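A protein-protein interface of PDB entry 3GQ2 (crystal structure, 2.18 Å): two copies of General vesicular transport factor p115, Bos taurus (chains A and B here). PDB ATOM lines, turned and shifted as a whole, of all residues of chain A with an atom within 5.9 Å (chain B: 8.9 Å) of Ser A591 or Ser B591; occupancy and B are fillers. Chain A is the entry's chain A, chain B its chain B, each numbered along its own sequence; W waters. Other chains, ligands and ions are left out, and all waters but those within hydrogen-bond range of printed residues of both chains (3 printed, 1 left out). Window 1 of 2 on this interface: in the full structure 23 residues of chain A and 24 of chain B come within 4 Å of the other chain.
Of the printed residues of chain B, His A587 touches Ser B591 and Gln B595.
Printed residues of chain B within 4 Å of Glu A588: Glu B588, Arg B592 and Gln B595.
Of chain B, only Ser B585 (3.5 Å), Lys B586 (3.1 Å), His B587 (3.0 Å), Tyr B590 (3.9 Å) and Ser B591 (2.5 Å) come within 4 Å of Ser A591.
Ser A594 touches just one residue of chain B: Lys B586.
Of chain A, only Ser A585, Lys A586, His A587, Tyr A590 and Ser A591 come within 4 Å of Ser B591.
Of the printed residues of chain A, Ser B594 touches Lys A586.
The nearest residue of chain A that does not touch Ser B591 is Glu A588 (4.1 Å).
The nearest printed residue of chain B that does not touch Ser A585 is Ser B594 (4.5 Å).
The backbone carbonyl oxygen (O) of Ser A585 sits at hydrogen-bond distance from the side-chain hydroxyl (OG) of Ser B591 (3.3 Å).
The side-chain amide nitrogen (NE2) of Gln B595 sits at hydrogen-bond distance from the backbone carbonyl oxygen (O) of Lys A586 (2.7 Å).
The side-chain carboxylate (OE1) of Glu A588 is in hydrogen-bond range of the side-chain amide nitrogen (NE2) of Gln B595 (3.0 Å).
O of His B587 sits close to OG of Ser A591 (3.3 Å).
The side-chain hydroxyl (OG) of Ser A591 sits at hydrogen-bond distance from the side-chain hydroxyl (OG) of Ser B591 (2.5 Å).
The side-chain carboxylate of Glu B588 lies within salt-bridge range of the guanidinium group of Arg A592 (3.5 Å).
O of Lys B586 lies within hydrogen-bond range of NE2 of Gln A595, 2.7 Å away.
The side-chain amide nitrogen (NE2) of Gln A595 sits close to the backbone NH (N) of Glu B588 (3.4 Å).
The backbone carbonyl oxygen (O) of Lys A586 sits close to the backbone carbonyl oxygen (O) of Ser B591 (3.2 Å).
O of Lys B586 sits close to O of Ser A591, at 3.1 Å.
A ring nitrogen (ND1) of His A587 sits close to the backbone NH (N) of Leu A589 (3.2 Å).
The side-chain hydroxyl (OG) of Ser A594 sits at hydrogen-bond distance from the backbone carbonyl oxygen (O) of Ser A591 (2.6 Å).
The side-chain hydroxyl of Ser B585 sits at hydrogen-bond distance from the backbone carbonyl oxygen of Gly B582, 3.5 Å away.
O of Gly B582 is in hydrogen-bond range of NZ of Lys B586, 3.1 Å away.
The backbone carbonyl oxygen of Thr B614 lies within hydrogen-bond range of the side-chain hydroxyl of Tyr B590 (3.0 Å).
OG of Ser B594 sits at hydrogen-bond distance from O of Ser B591 (2.4 Å).
Lys A586 touches Ser B591, and with the chains exchanged Ser A591 touches Lys B586.
His A587 touches Ser B591, and with the chains exchanged Ser A591 touches His B587.
Glu A588 touches Arg B592, and with the chains exchanged Arg A592 touches Glu B588.
Ser B591 touches its own counterpart, Ser A591.
Of the 20 pairs that touch across the chains among the printed residues, 20 have their exchanged pair printed and touching as well.
Water W3 lies within hydrogen-bond range of the backbone carbonyl oxygen (O) of Glu A588 (2.6 Å), the backbone carbonyl oxygen (O) of Glu B588 (2.6 Å) and the backbone NH (N) of Arg A592 (3.2 Å).
Water W1 bridges the guanidinium group (NH1) of Arg A592 and the side-chain carboxylate (OE2) of Glu B588.
Water W2 lies within hydrogen-bond range of the backbone carbonyl oxygen of Ser A585 (2.7 Å) and the side-chain hydroxyl of Ser B591 (3.4 Å).
Hydrophobic or aromatic side chains of chain B within 4 Å of the printed part of chain A: Tyr B590.
Of the 11 printed residues of chain A, 9 touch a printed residue of chain B.
Printed residues of chain A that touch a printed residue of chain B: Ser A585, Lys A586, His A587, Glu A588, Tyr A590, Ser A591, Arg A592, Ser A594 and Gln A595.
Hydrophobic or aromatic side chains of chain A that line the printed part of chain B: Tyr A590.
Among the printed residues, Asp or Glu carboxylates within 4 Å of a Lys or Arg side-chain nitrogen of the other chain: Arg A592 with Glu B588 (3.5 Å).
Among the printed residues, pairs that only touch across the chains: Glu A588 with Arg B592 (3.1 Å), His A587 with Ser B591 (3.2 Å), Ser A591 with Ser B585 (3.5 Å), Ser A594 with Lys B586 (3.6 Å), Lys A586 with Ser B594 (3.7 Å), Tyr A590 with Ser B591 (3.7 Å), His A587 with Gln B595 (3.8 Å), Gln A595 with His B587 (3.9 Å), Ser A591 with Tyr B590 (3.9 Å) and Glu A588 with Glu B588 (3.97 Å).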
ATOM      1  N   SER A 585      15.391  33.910  -4.924  1.00  0.00           N
ATOM      2  CA  SER A 585      14.904  32.562  -4.547  1.00  0.00           C
ATOM      3  C   SER A 585      15.877  31.743  -3.691  1.00  0.00           C
ATOM      4  O   SER A 585      15.487  30.736  -3.088  1.00  0.00           O
ATOM      5  CB  SER A 585      14.609  31.760  -5.804  1.00  0.00           C
ATOM      6  OG  SER A 585      15.786  31.588  -6.575  1.00  0.00           O
ATOM      7  N   LYS A 586      17.149  32.145  -3.655  1.00  0.00           N
ATOM      8  CA  LYS A 586      18.183  31.370  -2.979  1.00  0.00           C
ATOM      9  C   LYS A 586      18.427  31.832  -1.548  1.00  0.00           C
ATOM     10  O   LYS A 586      19.162  31.176  -0.777  1.00  0.00           O
ATOM     11  CB  LYS A 586      19.489  31.446  -3.768  1.00  0.00           C
ATOM     12  CG  LYS A 586      19.441  30.661  -5.074  1.00  0.00           C
ATOM     13  CD  LYS A 586      20.788  30.594  -5.715  1.00  0.00           C
ATOM     14  CE  LYS A 586      20.774  29.694  -6.960  1.00  0.00           C
ATOM     15  NZ  LYS A 586      20.680  30.472  -8.237  1.00  0.00           N
ATOM     16  N   HIS A 587      17.819  32.952  -1.178  1.00  0.00           N
ATOM     17  CA  HIS A 587      18.018  33.520   0.145  1.00  0.00           C
ATOM     18  C   HIS A 587      17.442  32.572   1.186  1.00  0.00           C
ATOM     19  O   HIS A 587      16.382  32.011   0.991  1.00  0.00           O
ATOM     20  CB  HIS A 587      17.400  34.926   0.219  1.00  0.00           C
ATOM     21  CG  HIS A 587      17.659  35.623   1.517  1.00  0.00           C
ATOM     22  ND1 HIS A 587      17.013  35.280   2.681  1.00  0.00           N
ATOM     23  CD2 HIS A 587      18.511  36.624   1.840  1.00  0.00           C
ATOM     24  CE1 HIS A 587      17.464  36.027   3.674  1.00  0.00           C
ATOM     25  NE2 HIS A 587      18.375  36.851   3.191  1.00  0.00           N
ATOM     26  N   GLU A 588      18.143  32.383   2.297  1.00  0.00           N
ATOM     27  CA  GLU A 588      17.760  31.361   3.266  1.00  0.00           C
ATOM     28  C   GLU A 588      16.286  31.420   3.769  1.00  0.00           C
ATOM     29  O   GLU A 588      15.724  30.426   4.193  1.00  0.00           O
ATOM     30  CB  GLU A 588      18.745  31.336   4.447  1.00  0.00           C
ATOM     31  CG  GLU A 588      19.019  32.678   5.180  1.00  0.00           C
ATOM     32  CD  GLU A 588      20.136  33.556   4.537  1.00  0.00           C
ATOM     33  OE1 GLU A 588      20.596  33.292   3.386  1.00  0.00           O
ATOM     34  OE2 GLU A 588      20.533  34.542   5.191  1.00  0.00           O
ATOM     35  N   LEU A 589      15.666  32.580   3.702  1.00  0.00           N
ATOM     36  CA  LEU A 589      14.377  32.794   4.314  1.00  0.00           C
ATOM     37  C   LEU A 589      13.282  32.719   3.285  1.00  0.00           C
ATOM     38  O   LEU A 589      12.097  32.798   3.618  1.00  0.00           O
ATOM     39  CB  LEU A 589      14.364  34.183   5.004  1.00  0.00           C
ATOM     40  CG  LEU A 589      15.133  34.272   6.331  1.00  0.00           C
ATOM     41  CD1 LEU A 589      14.865  35.575   6.994  1.00  0.00           C
ATOM     42  CD2 LEU A 589      14.783  33.111   7.273  1.00  0.00           C
ATOM     43  N   TYR A 590      13.683  32.603   2.023  1.00  0.00           N
ATOM     44  CA  TYR A 590      12.745  32.557   0.921  1.00  0.00           C
ATOM     45  C   TYR A 590      11.760  31.351   0.944  1.00  0.00           C
ATOM     46  O   TYR A 590      10.569  31.582   0.991  1.00  0.00           O
ATOM     47  CB  TYR A 590      13.510  32.637  -0.383  1.00  0.00           C
ATOM     48  CG  TYR A 590      12.638  32.629  -1.598  1.00  0.00           C
ATOM     49  CD1 TYR A 590      12.102  33.812  -2.095  1.00  0.00           C
ATOM     50  CD2 TYR A 590      12.327  31.425  -2.247  1.00  0.00           C
ATOM     51  CE1 TYR A 590      11.299  33.802  -3.191  1.00  0.00           C
ATOM     52  CE2 TYR A 590      11.533  31.411  -3.321  1.00  0.00           C
ATOM     53  CZ  TYR A 590      11.021  32.608  -3.810  1.00  0.00           C
ATOM     54  OH  TYR A 590      10.235  32.597  -4.923  1.00  0.00           O
ATOM     55  N   SER A 591      12.210  30.092   0.940  1.00  0.00           N
ATOM     56  CA  SER A 591      11.231  28.964   0.970  1.00  0.00           C
ATOM     57  C   SER A 591      10.197  29.004   2.072  1.00  0.00           C
ATOM     58  O   SER A 591       9.057  28.644   1.852  1.00  0.00           O
ATOM     59  CB  SER A 591      11.870  27.593   1.160  1.00  0.00           C
ATOM     60  OG  SER A 591      13.196  27.601   0.896  1.00  0.00           O
ATOM     61  N   ARG A 592      10.621  29.337   3.280  1.00  0.00           N
ATOM     62  CA  ARG A 592       9.717  29.402   4.405  1.00  0.00           C
ATOM     63  C   ARG A 592       8.600  30.411   4.155  1.00  0.00           C
ATOM     64  O   ARG A 592       7.442  30.130   4.388  1.00  0.00           O
ATOM     65  CB  ARG A 592      10.478  29.768   5.675  1.00  0.00           C
ATOM     66  CG  ARG A 592       9.595  29.870   6.903  1.00  0.00           C
ATOM     67  CD  ARG A 592      10.402  29.968   8.185  1.00  0.00           C
ATOM     68  NE  ARG A 592       9.961  28.937   9.122  1.00  0.00           N
ATOM     69  CZ  ARG A 592      10.700  27.924   9.575  1.00  0.00           C
ATOM     70  NH1 ARG A 592      11.980  27.804   9.242  1.00  0.00           N
ATOM     71  NH2 ARG A 592      10.155  27.037  10.404  1.00  0.00           N
ATOM     72  N   ALA A 593       8.949  31.583   3.651  1.00  0.00           N
ATOM     73  CA  ALA A 593       7.945  32.600   3.377  1.00  0.00           C
ATOM     74  C   ALA A 593       6.979  32.136   2.303  1.00  0.00           C
ATOM     75  O   ALA A 593       5.823  32.580   2.271  1.00  0.00           O
ATOM     76  CB  ALA A 593       8.600  33.880   2.965  1.00  0.00           C
ATOM     77  N   SER A 594       7.447  31.229   1.446  1.00  0.00           N
ATOM     78  CA  SER A 594       6.654  30.759   0.318  1.00  0.00           C
ATOM     79  C   SER A 594       5.627  29.709   0.721  1.00  0.00           C
ATOM     80  O   SER A 594       4.837  29.313  -0.110  1.00  0.00           O
ATOM     81  CB  SER A 594       7.560  30.170  -0.768  1.00  0.00           C
ATOM     82  OG  SER A 594       7.938  28.804  -0.463  1.00  0.00           O
ATOM     83  N   GLN A 595       5.661  29.231   1.963  1.00  0.00           N
ATOM     84  CA  GLN A 595       4.795  28.158   2.400  1.00  0.00           C
ATOM     85  C   GLN A 595       3.348  28.581   2.514  1.00  0.00           C
ATOM     86  O   GLN A 595       2.474  27.899   1.960  1.00  0.00           O
ATOM     87  CB  GLN A 595       5.223  27.603   3.768  1.00  0.00           C
ATOM     88  CG  GLN A 595       6.518  26.867   3.728  1.00  0.00           C
ATOM     89  CD  GLN A 595       6.981  26.359   5.062  1.00  0.00           C
ATOM     90  OE1 GLN A 595       6.294  26.488   6.063  1.00  0.00           O
ATOM     91  NE2 GLN A 595       8.163  25.721   5.072  1.00  0.00           N
ATOM     92  N   GLY B 582       5.072  19.986  -4.675  1.00  0.00           N
ATOM     93  CA  GLY B 582       5.433  21.347  -4.268  1.00  0.00           C
ATOM     94  C   GLY B 582       5.964  21.528  -2.849  1.00  0.00           C
ATOM     95  O   GLY B 582       6.587  22.563  -2.564  1.00  0.00           O
ATOM     96  N   PHE B 583       5.734  20.545  -1.961  1.00  0.00           N
ATOM     97  CA  PHE B 583       6.285  20.603  -0.595  1.00  0.00           C
ATOM     98  C   PHE B 583       7.809  20.603  -0.585  1.00  0.00           C
ATOM     99  O   PHE B 583       8.423  21.101   0.360  1.00  0.00           O
ATOM    100  CB  PHE B 583       5.814  19.439   0.304  1.00  0.00           C
ATOM    101  CG  PHE B 583       4.327  19.383   0.561  1.00  0.00           C
ATOM    102  CD1 PHE B 583       3.759  18.213   1.058  1.00  0.00           C
ATOM    103  CD2 PHE B 583       3.497  20.470   0.350  1.00  0.00           C
ATOM    104  CE1 PHE B 583       2.385  18.123   1.331  1.00  0.00           C
ATOM    105  CE2 PHE B 583       2.108  20.372   0.610  1.00  0.00           C
ATOM    106  CZ  PHE B 583       1.564  19.199   1.093  1.00  0.00           C
ATOM    107  N   ILE B 584       8.446  20.041  -1.609  1.00  0.00           N
ATOM    108  CA  ILE B 584       9.893  19.929  -1.564  1.00  0.00           C
ATOM    109  C   ILE B 584      10.507  21.343  -1.570  1.00  0.00           C
ATOM    110  O   ILE B 584      11.279  21.724  -0.702  1.00  0.00           O
ATOM    111  CB  ILE B 584      10.482  19.084  -2.758  1.00  0.00           C
ATOM    112  CG1 ILE B 584       9.737  17.744  -2.948  1.00  0.00           C
ATOM    113  CG2 ILE B 584      11.979  18.829  -2.501  1.00  0.00           C
ATOM    114  CD1 ILE B 584       9.880  17.146  -4.367  1.00  0.00           C
ATOM    115  N   SER B 585      10.164  22.121  -2.575  1.00  0.00           N
ATOM    116  CA  SER B 585      10.755  23.448  -2.695  1.00  0.00           C
ATOM    117  C   SER B 585      10.292  24.464  -1.612  1.00  0.00           C
ATOM    118  O   SER B 585      10.966  25.446  -1.387  1.00  0.00           O
ATOM    119  CB  SER B 585      10.497  24.003  -4.078  1.00  0.00           C
ATOM    120  OG  SER B 585       9.126  24.259  -4.261  1.00  0.00           O
ATOM    121  N   LYS B 586       9.165  24.209  -0.955  1.00  0.00           N
ATOM    122  CA  LYS B 586       8.669  25.101   0.108  1.00  0.00           C
ATOM    123  C   LYS B 586       9.191  24.794   1.520  1.00  0.00           C
ATOM    124  O   LYS B 586       9.002  25.607   2.477  1.00  0.00           O
ATOM    125  CB  LYS B 586       7.148  25.089   0.119  1.00  0.00           C
ATOM    126  CG  LYS B 586       6.567  25.592  -1.182  1.00  0.00           C
ATOM    127  CD  LYS B 586       5.047  25.718  -1.081  1.00  0.00           C
ATOM    128  CE  LYS B 586       4.429  25.937  -2.432  1.00  0.00           C
ATOM    129  NZ  LYS B 586       4.473  24.704  -3.272  1.00  0.00           N
ATOM    130  N   HIS B 587       9.871  23.645   1.662  1.00  0.00           N
ATOM    131  CA  HIS B 587      10.454  23.279   2.940  1.00  0.00           C
ATOM    132  C   HIS B 587      11.384  24.389   3.386  1.00  0.00           C
ATOM    133  O   HIS B 587      12.160  24.953   2.587  1.00  0.00           O
ATOM    134  CB  HIS B 587      11.173  21.928   2.855  1.00  0.00           C
ATOM    135  CG  HIS B 587      11.546  21.377   4.186  1.00  0.00           C
ATOM    136  ND1 HIS B 587      12.658  21.812   4.869  1.00  0.00           N
ATOM    137  CD2 HIS B 587      10.923  20.489   5.000  1.00  0.00           C
ATOM    138  CE1 HIS B 587      12.716  21.208   6.047  1.00  0.00           C
ATOM    139  NE2 HIS B 587      11.673  20.401   6.154  1.00  0.00           N
ATOM    140  N   GLU B 588      11.342  24.700   4.680  1.00  0.00           N
ATOM    141  CA  GLU B 588      12.016  25.864   5.164  1.00  0.00           C
ATOM    142  C   GLU B 588      13.523  25.805   4.899  1.00  0.00           C
ATOM    143  O   GLU B 588      14.167  26.840   4.894  1.00  0.00           O
ATOM    144  CB  GLU B 588      11.754  26.098   6.663  1.00  0.00           C
ATOM    145  CG  GLU B 588      12.219  24.994   7.625  1.00  0.00           C
ATOM    146  CD  GLU B 588      11.070  24.104   8.151  1.00  0.00           C
ATOM    147  OE1 GLU B 588      10.146  23.689   7.359  1.00  0.00           O
ATOM    148  OE2 GLU B 588      11.135  23.813   9.377  1.00  0.00           O
ATOM    149  N   LEU B 589      14.062  24.601   4.677  1.00  0.00           N
ATOM    150  CA  LEU B 589      15.508  24.414   4.562  1.00  0.00           C
ATOM    151  C   LEU B 589      16.014  24.370   3.139  1.00  0.00           C
ATOM    152  O   LEU B 589      17.215  24.347   2.911  1.00  0.00           O
ATOM    153  CB  LEU B 589      15.966  23.122   5.269  1.00  0.00           C
ATOM    154  CG  LEU B 589      15.865  23.145   6.801  1.00  0.00           C
ATOM    155  CD1 LEU B 589      16.271  21.800   7.383  1.00  0.00           C
ATOM    156  CD2 LEU B 589      16.686  24.266   7.364  1.00  0.00           C
ATOM    157  N   TYR B 590      15.111  24.363   2.182  1.00  0.00           N
ATOM    158  CA  TYR B 590      15.479  24.145   0.798  1.00  0.00           C
ATOM    159  C   TYR B 590      16.311  25.287   0.260  1.00  0.00           C
ATOM    160  O   TYR B 590      17.421  25.061  -0.242  1.00  0.00           O
ATOM    161  CB  TYR B 590      14.218  23.950  -0.009  1.00  0.00           C
ATOM    162  CG  TYR B 590      14.376  23.792  -1.499  1.00  0.00           C
ATOM    163  CD1 TYR B 590      14.421  22.525  -2.099  1.00  0.00           C
ATOM    164  CD2 TYR B 590      14.423  24.907  -2.317  1.00  0.00           C
ATOM    165  CE1 TYR B 590      14.552  22.397  -3.476  1.00  0.00           C
ATOM    166  CE2 TYR B 590      14.543  24.793  -3.664  1.00  0.00           C
ATOM    167  CZ  TYR B 590      14.608  23.542  -4.253  1.00  0.00           C
ATOM    168  OH  TYR B 590      14.730  23.489  -5.619  1.00  0.00           O
ATOM    169  N   SER B 591      15.784  26.507   0.344  1.00  0.00           N
ATOM    170  CA  SER B 591      16.509  27.666  -0.184  1.00  0.00           C
ATOM    171  C   SER B 591      17.987  27.725   0.163  1.00  0.00           C
ATOM    172  O   SER B 591      18.847  27.957  -0.693  1.00  0.00           O
ATOM    173  CB  SER B 591      15.869  28.964   0.334  1.00  0.00           C
ATOM    174  OG  SER B 591      14.668  29.147  -0.327  1.00  0.00           O
ATOM    175  N   ARG B 592      18.276  27.611   1.438  1.00  0.00           N
ATOM    176  CA  ARG B 592      19.649  27.684   1.915  1.00  0.00           C
ATOM    177  C   ARG B 592      20.474  26.616   1.191  1.00  0.00           C
ATOM    178  O   ARG B 592      21.506  26.926   0.645  1.00  0.00           O
ATOM    179  CB  ARG B 592      19.721  27.493   3.434  1.00  0.00           C
ATOM    180  CG  ARG B 592      21.037  27.945   4.121  1.00  0.00           C
ATOM    181  CD  ARG B 592      20.879  27.664   5.613  1.00  0.00           C
ATOM    182  NE  ARG B 592      21.852  28.284   6.499  1.00  0.00           N
ATOM    183  CZ  ARG B 592      21.795  29.535   6.954  1.00  0.00           C
ATOM    184  NH1 ARG B 592      20.809  30.350   6.596  1.00  0.00           N
ATOM    185  NH2 ARG B 592      22.752  29.982   7.771  1.00  0.00           N
ATOM    186  N   ALA B 593      19.967  25.395   1.129  1.00  0.00           N
ATOM    187  CA  ALA B 593      20.660  24.283   0.433  1.00  0.00           C
ATOM    188  C   ALA B 593      20.987  24.621  -1.021  1.00  0.00           C
ATOM    189  O   ALA B 593      21.999  24.219  -1.554  1.00  0.00           O
ATOM    190  CB  ALA B 593      19.813  23.054   0.469  1.00  0.00           C
ATOM    191  N   SER B 594      20.118  25.384  -1.651  1.00  0.00           N
ATOM    192  CA  SER B 594      20.283  25.768  -3.033  1.00  0.00           C
ATOM    193  C   SER B 594      21.366  26.799  -3.297  1.00  0.00           C
ATOM    194  O   SER B 594      21.618  27.153  -4.450  1.00  0.00           O
ATOM    195  CB  SER B 594      18.939  26.279  -3.534  1.00  0.00           C
ATOM    196  OG  SER B 594      18.684  27.598  -3.080  1.00  0.00           O
ATOM    197  N   GLN B 595      22.018  27.303  -2.262  1.00  0.00           N
ATOM    198  CA  GLN B 595      22.910  28.450  -2.441  1.00  0.00           C
ATOM    199  C   GLN B 595      24.296  28.064  -2.909  1.00  0.00           C
ATOM    200  O   GLN B 595      24.891  28.765  -3.725  1.00  0.00           O
ATOM    201  CB  GLN B 595      23.080  29.233  -1.134  1.00  0.00           C
ATOM    202  CG  GLN B 595      21.883  30.049  -0.716  1.00  0.00           C
ATOM    203  CD  GLN B 595      22.053  30.689   0.666  1.00  0.00           C
ATOM    204  OE1 GLN B 595      23.042  30.463   1.349  1.00  0.00           O
ATOM    205  NE2 GLN B 595      21.079  31.489   1.074  1.00  0.00           N
ATOM    206  N   LYS B 596      24.841  26.990  -2.350  1.00  0.00           N
ATOM    207  CA  LYS B 596      26.193  26.587  -2.701  1.00  0.00           C
ATOM    208  C   LYS B 596      26.369  25.107  -2.451  1.00  0.00           C
ATOM    209  O   LYS B 596      25.506  24.500  -1.874  1.00  0.00           O
ATOM    210  CB  LYS B 596      27.242  27.419  -1.943  1.00  0.00           C
ATOM    211  CG  LYS B 596      27.224  27.301  -0.428  1.00  0.00           C
ATOM    212  CD  LYS B 596      28.098  28.386   0.181  1.00  0.00           C
ATOM    213  CE  LYS B 596      27.898  28.501   1.686  1.00  0.00           C
ATOM    214  NZ  LYS B 596      28.163  27.199   2.394  1.00  0.00           N
ATOM    215  N   ASN B 600      25.731  23.043   4.611  1.00  0.00           N
ATOM    216  CA  ASN B 600      25.503  24.233   5.419  1.00  0.00           C
ATOM    217  C   ASN B 600      24.426  23.899   6.453  1.00  0.00           C
ATOM    218  O   ASN B 600      23.249  24.287   6.311  1.00  0.00           O
ATOM    219  CB  ASN B 600      25.064  25.367   4.496  1.00  0.00           C
ATOM    220  CG  ASN B 600      24.999  26.704   5.179  1.00  0.00           C
ATOM    221  OD1 ASN B 600      25.107  26.811   6.406  1.00  0.00           O
ATOM    222  ND2 ASN B 600      24.804  27.758   4.374  1.00  0.00           N
ATOM    223  N   PHE B 609      18.769  18.407   3.165  1.00  0.00           N
ATOM    224  CA  PHE B 609      18.852  18.594   1.704  1.00  0.00           C
ATOM    225  C   PHE B 609      20.274  18.512   1.222  1.00  0.00           C
ATOM    226  O   PHE B 609      21.186  18.890   1.938  1.00  0.00           O
ATOM    227  CB  PHE B 609      18.318  19.953   1.269  1.00  0.00           C
ATOM    228  CG  PHE B 609      16.817  20.024   1.214  1.00  0.00           C
ATOM    229  CD1 PHE B 609      16.116  19.295   0.281  1.00  0.00           C
ATOM    230  CD2 PHE B 609      16.113  20.834   2.087  1.00  0.00           C
ATOM    231  CE1 PHE B 609      14.741  19.329   0.262  1.00  0.00           C
ATOM    232  CE2 PHE B 609      14.731  20.881   2.054  1.00  0.00           C
ATOM    233  CZ  PHE B 609      14.042  20.132   1.123  1.00  0.00           C
ATOM    234  N   HIS B 611      22.854  19.737  -1.967  1.00  0.00           N
ATOM    235  CA  HIS B 611      22.816  20.883  -2.891  1.00  0.00           C
ATOM    236  C   HIS B 611      22.494  20.469  -4.323  1.00  0.00           C
ATOM    237  O   HIS B 611      21.645  21.102  -4.968  1.00  0.00           O
ATOM    238  CB  HIS B 611      24.108  21.650  -2.834  1.00  0.00           C
ATOM    239  CG  HIS B 611      24.250  22.681  -3.896  1.00  0.00           C
ATOM    240  ND1 HIS B 611      23.443  23.799  -3.970  1.00  0.00           N
ATOM    241  CD2 HIS B 611      25.117  22.774  -4.923  1.00  0.00           C
ATOM    242  CE1 HIS B 611      23.808  24.532  -5.005  1.00  0.00           C
ATOM    243  NE2 HIS B 611      24.834  23.944  -5.591  1.00  0.00           N
ATOM    244  N   THR B 614      18.866  19.822  -4.855  1.00  0.00           N
ATOM    245  CA  THR B 614      17.962  20.961  -5.052  1.00  0.00           C
ATOM    246  C   THR B 614      17.943  21.355  -6.511  1.00  0.00           C
ATOM    247  O   THR B 614      16.916  21.866  -6.982  1.00  0.00           O
ATOM    248  CB  THR B 614      18.318  22.218  -4.270  1.00  0.00           C
ATOM    249  OG1 THR B 614      19.537  22.787  -4.796  1.00  0.00           O
ATOM    250  CG2 THR B 614      18.414  21.931  -2.763  1.00  0.00           C
HETATM  251  O   HOH W   1      12.377  25.741  10.740  1.00  0.00           O
HETATM  252  O   HOH W   2      14.296  28.361  -3.620  1.00  0.00           O
HETATM  253  O   HOH W   3      13.487  29.346   4.789  1.00  0.00           O
